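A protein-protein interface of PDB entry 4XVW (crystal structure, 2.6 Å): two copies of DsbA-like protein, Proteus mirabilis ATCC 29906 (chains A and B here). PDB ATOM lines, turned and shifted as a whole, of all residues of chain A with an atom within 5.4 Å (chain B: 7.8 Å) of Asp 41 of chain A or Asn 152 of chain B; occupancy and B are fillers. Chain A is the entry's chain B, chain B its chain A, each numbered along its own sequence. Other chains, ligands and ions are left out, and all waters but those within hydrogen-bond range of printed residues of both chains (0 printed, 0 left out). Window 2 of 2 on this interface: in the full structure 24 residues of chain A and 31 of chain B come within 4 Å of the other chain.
No position is printed for both chains.
Thr 37 of chain A touches Glu 116 of chain B (CA to OE2, 3.4 Å). Lys 120 of chain B touches Thr 37 of chain A (CD to CG2, 3.6 Å). CB of Ala 40 of chain A touches CD of Glu 116 of chain B (3.5 Å). Gln 44 of chain A touches Asp 151 of chain B.
Of the 16 printed residues of chain B, 4 touch a printed residue of chain A. Of the 9 printed residues of chain A, 4 touch a printed residue of chain B. Printed residues of chain A that touch a printed residue of chain B: Thr 37, Ala 40, Asp 41 and Gln 44. Among the printed residues, 7 pairs touch across the chains. Among the printed residues, Asp or Glu carboxylates within 4 Å of a Lys or Arg side-chain nitrogen of the other chain: Asp 41 of chain A with Lys 120 of chain B (3.3 Å).
Asp 41 of chain A touches two residues of chain B. Asn 152 of chain B touches just these residues of chain A: Asp 41 and Gln 44. Printed residues of chain B within 4 Å of Ala 40 of chain A: Glu 116 (3.5 Å). Of the printed residues of chain B, Gln 44 of chain A touches Asp 151 (3.5 Å) and Asn 152 (3.1 Å). Of the printed residues of chain A, Glu 116 of chain B touches Thr 37 (3.4 Å) and Ala 40 (3.5 Å). Of the printed residues of chain A, Lys 120 of chain B touches Thr 37 (3.6 Å) and Asp 41 (3.3 Å). Of the printed residues of chain A, Asp 151 of chain B touches Gln 44 (3.5 Å). Printed residues of chain B within 4 Å of Thr 37 of chain A: Glu 116 and Lys 120. Ala 45 of chain A touches none of the printed residues of chain B. Ser 117 of chain B touches none of the printed residues of chain A.
OD1 of Asp 151 of chain B sits close to N of Ala 153 of chain B (3.2 Å). The backbone NH (N) of Ser 154 of chain B lies within hydrogen-bond range of the side-chain carboxylate (OD1) of Asp 151 of chain B, at 2.5 Å.
OD2 of Asp 41 of chain A lies within salt-bridge range of NZ of Lys 120 of chain B (3.3 Å). ND2 of Asn 152 of chain B sits at hydrogen-bond distance from OD1 of Asp 41 of chain A, at 2.8 Å. OE1 of Gln 44 of chain A sits close to N of Asn 152 of chain B (3.3 Å).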
ATOM      1  N   THR A  37       0.961  20.181  -4.060  1.00  0.00           N
ATOM      2  CA  THR A  37       1.210  20.873  -2.804  1.00  0.00           C
ATOM      3  C   THR A  37       2.710  20.898  -2.548  1.00  0.00           C
ATOM      4  O   THR A  37       3.272  21.926  -2.175  1.00  0.00           O
ATOM      5  CB  THR A  37       0.476  20.197  -1.628  1.00  0.00           C
ATOM      6  OG1 THR A  37      -0.939  20.331  -1.804  1.00  0.00           O
ATOM      7  CG2 THR A  37       0.882  20.819  -0.299  1.00  0.00           C
ATOM      8  N   LYS A  38       3.348  19.749  -2.745  1.00  0.00           N
ATOM      9  CA  LYS A  38       4.782  19.623  -2.536  1.00  0.00           C
ATOM     10  C   LYS A  38       5.554  20.511  -3.500  1.00  0.00           C
ATOM     11  O   LYS A  38       6.597  21.052  -3.145  1.00  0.00           O
ATOM     12  CB  LYS A  38       5.226  18.169  -2.704  1.00  0.00           C
ATOM     13  CG  LYS A  38       6.717  17.945  -2.485  1.00  0.00           C
ATOM     14  CD  LYS A  38       7.069  16.467  -2.539  1.00  0.00           C
ATOM     15  CE  LYS A  38       8.550  16.238  -2.290  1.00  0.00           C
ATOM     16  NZ  LYS A  38       9.386  16.772  -3.403  1.00  0.00           N
ATOM     17  N   LYS A  39       5.041  20.665  -4.716  1.00  0.00           N
ATOM     18  CA  LYS A  39       5.673  21.552  -5.684  1.00  0.00           C
ATOM     19  C   LYS A  39       5.647  22.990  -5.187  1.00  0.00           C
ATOM     20  O   LYS A  39       6.659  23.681  -5.223  1.00  0.00           O
ATOM     21  CB  LYS A  39       4.977  21.463  -7.046  1.00  0.00           C
ATOM     22  CG  LYS A  39       5.265  20.191  -7.830  1.00  0.00           C
ATOM     23  CD  LYS A  39       4.539  20.204  -9.168  1.00  0.00           C
ATOM     24  CE  LYS A  39       4.858  18.972 -10.001  1.00  0.00           C
ATOM     25  NZ  LYS A  39       4.099  18.950 -11.286  1.00  0.00           N
ATOM     26  N   ALA A  40       4.493  23.419  -4.684  1.00  0.00           N
ATOM     27  CA  ALA A  40       4.313  24.792  -4.224  1.00  0.00           C
ATOM     28  C   ALA A  40       5.157  25.077  -2.988  1.00  0.00           C
ATOM     29  O   ALA A  40       5.593  26.207  -2.768  1.00  0.00           O
ATOM     30  CB  ALA A  40       2.845  25.061  -3.932  1.00  0.00           C
ATOM     31  N   ASP A  41       5.391  24.042  -2.189  1.00  0.00           N
ATOM     32  CA  ASP A  41       6.197  24.170  -0.980  1.00  0.00           C
ATOM     33  C   ASP A  41       7.643  24.479  -1.336  1.00  0.00           C
ATOM     34  O   ASP A  41       8.355  25.140  -0.579  1.00  0.00           O
ATOM     35  CB  ASP A  41       6.127  22.885  -0.152  1.00  0.00           C
ATOM     36  CG  ASP A  41       4.748  22.634   0.426  1.00  0.00           C
ATOM     37  OD1 ASP A  41       3.907  23.558   0.398  1.00  0.00           O
ATOM     38  OD2 ASP A  41       4.505  21.509   0.911  1.00  0.00           O
ATOM     39  N   GLU A  42       8.070  23.996  -2.498  1.00  0.00           N
ATOM     40  CA  GLU A  42       9.430  24.206  -2.972  1.00  0.00           C
ATOM     41  C   GLU A  42       9.584  25.580  -3.613  1.00  0.00           C
ATOM     42  O   GLU A  42      10.603  26.247  -3.437  1.00  0.00           O
ATOM     43  CB  GLU A  42       9.794  23.108  -3.975  1.00  0.00           C
ATOM     44  CG  GLU A  42       9.748  21.704  -3.377  1.00  0.00           C
ATOM     45  CD  GLU A  42       9.840  20.604  -4.418  1.00  0.00           C
ATOM     46  OE1 GLU A  42       9.592  20.881  -5.608  1.00  0.00           O
ATOM     47  OE2 GLU A  42      10.147  19.454  -4.038  1.00  0.00           O
ATOM     48  N   GLN A  43       8.555  26.011  -4.334  1.00  0.00           N
ATOM     49  CA  GLN A  43       8.564  27.317  -4.981  1.00  0.00           C
ATOM     50  C   GLN A  43       8.551  28.433  -3.940  1.00  0.00           C
ATOM     51  O   GLN A  43       9.106  29.509  -4.174  1.00  0.00           O
ATOM     52  CB  GLN A  43       7.378  27.451  -5.935  1.00  0.00           C
ATOM     53  CG  GLN A  43       7.339  26.355  -6.986  1.00  0.00           C
ATOM     54  CD  GLN A  43       6.164  26.475  -7.929  1.00  0.00           C
ATOM     55  OE1 GLN A  43       5.276  27.305  -7.733  1.00  0.00           O
ATOM     56  NE2 GLN A  43       6.133  25.618  -8.944  1.00  0.00           N
ATOM     57  N   GLN A  44       7.929  28.168  -2.792  1.00  0.00           N
ATOM     58  CA  GLN A  44       7.831  29.160  -1.724  1.00  0.00           C
ATOM     59  C   GLN A  44       8.845  28.871  -0.630  1.00  0.00           C
ATOM     60  O   GLN A  44       8.522  28.906   0.557  1.00  0.00           O
ATOM     61  CB  GLN A  44       6.435  29.180  -1.104  1.00  0.00           C
ATOM     62  CG  GLN A  44       5.303  29.503  -2.054  1.00  0.00           C
ATOM     63  CD  GLN A  44       3.947  29.270  -1.416  1.00  0.00           C
ATOM     64  OE1 GLN A  44       3.844  28.626  -0.372  1.00  0.00           O
ATOM     65  NE2 GLN A  44       2.900  29.797  -2.037  1.00  0.00           N
ATOM     66  N   ALA A  45      10.071  28.581  -1.044  1.00  0.00           N
ATOM     67  CA  ALA A  45      11.177  28.434  -0.117  1.00  0.00           C
ATOM     68  C   ALA A  45      12.019  29.680  -0.286  1.00  0.00           C
ATOM     69  O   ALA A  45      11.887  30.384  -1.285  1.00  0.00           O
ATOM     70  CB  ALA A  45      11.981  27.175  -0.403  1.00  0.00           C
ATOM     71  N   GLU B 116      -4.377  25.274  -5.033  1.00  0.00           N
ATOM     72  CA  GLU B 116      -3.504  24.451  -4.204  1.00  0.00           C
ATOM     73  C   GLU B 116      -3.504  24.941  -2.762  1.00  0.00           C
ATOM     74  O   GLU B 116      -3.396  24.149  -1.825  1.00  0.00           O
ATOM     75  CB  GLU B 116      -2.079  24.459  -4.768  1.00  0.00           C
ATOM     76  CG  GLU B 116      -1.053  23.696  -3.930  1.00  0.00           C
ATOM     77  CD  GLU B 116      -0.432  24.533  -2.819  1.00  0.00           C
ATOM     78  OE1 GLU B 116      -0.447  25.779  -2.914  1.00  0.00           O
ATOM     79  OE2 GLU B 116       0.073  23.939  -1.844  1.00  0.00           O
ATOM     80  N   SER B 117      -3.621  26.254  -2.592  1.00  0.00           N
ATOM     81  CA  SER B 117      -3.671  26.851  -1.266  1.00  0.00           C
ATOM     82  C   SER B 117      -4.899  26.359  -0.515  1.00  0.00           C
ATOM     83  O   SER B 117      -4.873  26.201   0.705  1.00  0.00           O
ATOM     84  CB  SER B 117      -3.682  28.376  -1.360  1.00  0.00           C
ATOM     85  OG  SER B 117      -4.856  28.838  -2.001  1.00  0.00           O
ATOM     86  N   LYS B 120      -4.053  23.135   0.879  1.00  0.00           N
ATOM     87  CA  LYS B 120      -3.122  23.321   1.982  1.00  0.00           C
ATOM     88  C   LYS B 120      -3.840  23.853   3.217  1.00  0.00           C
ATOM     89  O   LYS B 120      -3.598  23.395   4.333  1.00  0.00           O
ATOM     90  CB  LYS B 120      -2.006  24.282   1.568  1.00  0.00           C
ATOM     91  CG  LYS B 120      -0.817  24.323   2.514  1.00  0.00           C
ATOM     92  CD  LYS B 120      -0.001  23.042   2.438  1.00  0.00           C
ATOM     93  CE  LYS B 120       1.292  23.151   3.235  1.00  0.00           C
ATOM     94  NZ  LYS B 120       2.122  21.916   3.143  1.00  0.00           N
ATOM     95  N   ALA B 121      -4.727  24.821   3.006  1.00  0.00           N
ATOM     96  CA  ALA B 121      -5.506  25.402   4.093  1.00  0.00           C
ATOM     97  C   ALA B 121      -6.453  24.374   4.697  1.00  0.00           C
ATOM     98  O   ALA B 121      -6.619  24.306   5.915  1.00  0.00           O
ATOM     99  CB  ALA B 121      -6.285  26.606   3.594  1.00  0.00           C
ATOM    100  N   GLN B 123      -5.946  21.160   4.515  1.00  0.00           N
ATOM    101  CA  GLN B 123      -5.051  20.195   5.136  1.00  0.00           C
ATOM    102  C   GLN B 123      -4.674  20.644   6.542  1.00  0.00           C
ATOM    103  O   GLN B 123      -4.462  19.821   7.431  1.00  0.00           O
ATOM    104  CB  GLN B 123      -3.795  20.020   4.278  1.00  0.00           C
ATOM    105  CG  GLN B 123      -2.828  18.962   4.767  1.00  0.00           C
ATOM    106  CD  GLN B 123      -1.647  18.798   3.834  1.00  0.00           C
ATOM    107  OE1 GLN B 123      -1.514  19.528   2.853  1.00  0.00           O
ATOM    108  NE2 GLN B 123      -0.784  17.834   4.132  1.00  0.00           N
ATOM    109  N   LEU B 150      -4.381  32.807  -0.556  1.00  0.00           N
ATOM    110  CA  LEU B 150      -3.540  32.285   0.517  1.00  0.00           C
ATOM    111  C   LEU B 150      -2.268  31.637  -0.008  1.00  0.00           C
ATOM    112  O   LEU B 150      -2.232  31.112  -1.121  1.00  0.00           O
ATOM    113  CB  LEU B 150      -4.315  31.257   1.346  1.00  0.00           C
ATOM    114  CG  LEU B 150      -5.280  31.769   2.417  1.00  0.00           C
ATOM    115  CD1 LEU B 150      -6.417  32.582   1.824  1.00  0.00           C
ATOM    116  CD2 LEU B 150      -5.827  30.586   3.203  1.00  0.00           C
ATOM    117  N   ASP B 151      -1.226  31.692   0.813  1.00  0.00           N
ATOM    118  CA  ASP B 151       0.015  30.966   0.580  1.00  0.00           C
ATOM    119  C   ASP B 151       0.414  30.265   1.874  1.00  0.00           C
ATOM    120  O   ASP B 151      -0.280  30.382   2.880  1.00  0.00           O
ATOM    121  CB  ASP B 151       1.121  31.902   0.089  1.00  0.00           C
ATOM    122  CG  ASP B 151       1.247  33.153   0.931  1.00  0.00           C
ATOM    123  OD1 ASP B 151       0.926  33.102   2.135  1.00  0.00           O
ATOM    124  OD2 ASP B 151       1.669  34.193   0.386  1.00  0.00           O
ATOM    125  N   ASN B 152       1.529  29.544   1.853  1.00  0.00           N
ATOM    126  CA  ASN B 152       2.020  28.889   3.056  1.00  0.00           C
ATOM    127  C   ASN B 152       2.339  29.904   4.150  1.00  0.00           C
ATOM    128  O   ASN B 152       2.178  29.620   5.335  1.00  0.00           O
ATOM    129  CB  ASN B 152       3.265  28.054   2.743  1.00  0.00           C
ATOM    130  CG  ASN B 152       2.941  26.780   1.983  1.00  0.00           C
ATOM    131  OD1 ASN B 152       1.828  26.605   1.487  1.00  0.00           O
ATOM    132  ND2 ASN B 152       3.917  25.883   1.887  1.00  0.00           N
ATOM    133  N   ALA B 153       2.780  31.094   3.750  1.00  0.00           N
ATOM    134  CA  ALA B 153       3.101  32.149   4.708  1.00  0.00           C
ATOM    135  C   ALA B 153       1.857  32.708   5.393  1.00  0.00           C
ATOM    136  O   ALA B 153       1.832  32.856   6.614  1.00  0.00           O
ATOM    137  CB  ALA B 153       3.856  33.269   4.015  1.00  0.00           C
ATOM    138  N   SER B 154       0.825  33.006   4.609  1.00  0.00           N
ATOM    139  CA  SER B 154      -0.410  33.558   5.156  1.00  0.00           C
ATOM    140  C   SER B 154      -1.071  32.514   6.037  1.00  0.00           C
ATOM    141  O   SER B 154      -1.701  32.841   7.043  1.00  0.00           O
ATOM    142  CB  SER B 154      -1.361  34.001   4.041  1.00  0.00           C
ATOM    143  OG  SER B 154      -0.727  34.913   3.163  1.00  0.00           O
ATOM    144  N   ILE B 155      -0.923  31.253   5.649  1.00  0.00           N
ATOM    145  CA  ILE B 155      -1.466  30.160   6.434  1.00  0.00           C
ATOM    146  C   ILE B 155      -0.671  30.040   7.720  1.00  0.00           C
ATOM    147  O   ILE B 155      -1.248  29.940   8.796  1.00  0.00           O
ATOM    148  CB  ILE B 155      -1.427  28.824   5.661  1.00  0.00           C
ATOM    149  CG1 ILE B 155      -2.437  28.854   4.513  1.00  0.00           C
ATOM    150  CG2 ILE B 155      -1.756  27.651   6.583  1.00  0.00           C
ATOM    151  CD1 ILE B 155      -2.297  27.705   3.531  1.00  0.00           C
ATOM    152  N   GLU B 156       0.652  30.119   7.612  1.00  0.00           N
ATOM    153  CA  GLU B 156       1.523  29.960   8.771  1.00  0.00           C
ATOM    154  C   GLU B 156       1.399  31.152   9.710  1.00  0.00           C
ATOM    155  O   GLU B 156       1.772  31.069  10.880  1.00  0.00           O
ATOM    156  CB  GLU B 156       2.980  29.786   8.336  1.00  0.00           C
ATOM    157  CG  GLU B 156       3.340  28.373   7.901  1.00  0.00           C
ATOM    158  CD  GLU B 156       4.768  28.265   7.398  1.00  0.00           C
ATOM    159  OE1 GLU B 156       5.472  29.298   7.379  1.00  0.00           O
ATOM    160  OE2 GLU B 156       5.188  27.151   7.018  1.00  0.00           O
ATOM    161  N   ASP B 157       0.876  32.259   9.195  1.00  0.00           N
ATOM    162  CA  ASP B 157       0.679  33.448  10.009  1.00  0.00           C
ATOM    163  C   ASP B 157      -0.553  33.269  10.882  1.00  0.00           C
ATOM    164  O   ASP B 157      -0.585  33.707  12.030  1.00  0.00           O
ATOM    165  CB  ASP B 157       0.514  34.689   9.130  1.00  0.00           C
ATOM    166  CG  ASP B 157       1.810  35.125   8.477  1.00  0.00           C
ATOM    167  OD1 ASP B 157       2.892  34.812   9.016  1.00  0.00           O
ATOM    168  OD2 ASP B 157       1.744  35.779   7.417  1.00  0.00           O
ATOM    169  N   ALA B 158      -1.562  32.615  10.322  1.00  0.00           N
ATOM    170  CA  ALA B 158      -2.804  32.355  11.034  1.00  0.00           C
ATOM    171  C   ALA B 158      -2.685  31.238  12.074  1.00  0.00           C
ATOM    172  O   ALA B 158      -3.598  31.047  12.875  1.00  0.00           O
ATOM    173  CB  ALA B 158      -3.907  32.023  10.034  1.00  0.00           C
ATOM    174  N   MET B 159      -1.574  30.507  12.074  1.00  0.00           N
ATOM    175  CA  MET B 159      -1.472  29.313  12.909  1.00  0.00           C
ATOM    176  C   MET B 159      -1.118  29.615  14.392  1.00  0.00           C
ATOM    177  O   MET B 159      -1.980  29.402  15.253  1.00  0.00           O
ATOM    178  CB  MET B 159      -0.469  28.343  12.287  1.00  0.00           C
ATOM    179  CG  MET B 159      -0.921  27.694  10.979  1.00  0.00           C
ATOM    180  SD  MET B 159       0.053  26.086  10.463  1.00  0.00           S
ATOM    181  CE  MET B 159      -1.064  24.754  11.322  1.00  0.00           C
ATOM    182  N   LEU B 169       0.953  19.092   9.640  1.00  0.00           N
ATOM    183  CA  LEU B 169       0.037  18.777   8.553  1.00  0.00           C
ATOM    184  C   LEU B 169       0.257  17.335   8.117  1.00  0.00           C
ATOM    185  O   LEU B 169       1.270  17.007   7.498  1.00  0.00           O
ATOM    186  CB  LEU B 169       0.207  19.737   7.375  1.00  0.00           C
ATOM    187  CG  LEU B 169      -0.557  21.061   7.489  1.00  0.00           C
ATOM    188  CD1 LEU B 169      -0.068  21.923   8.643  1.00  0.00           C
ATOM    189  CD2 LEU B 169      -0.482  21.823   6.175  1.00  0.00           C
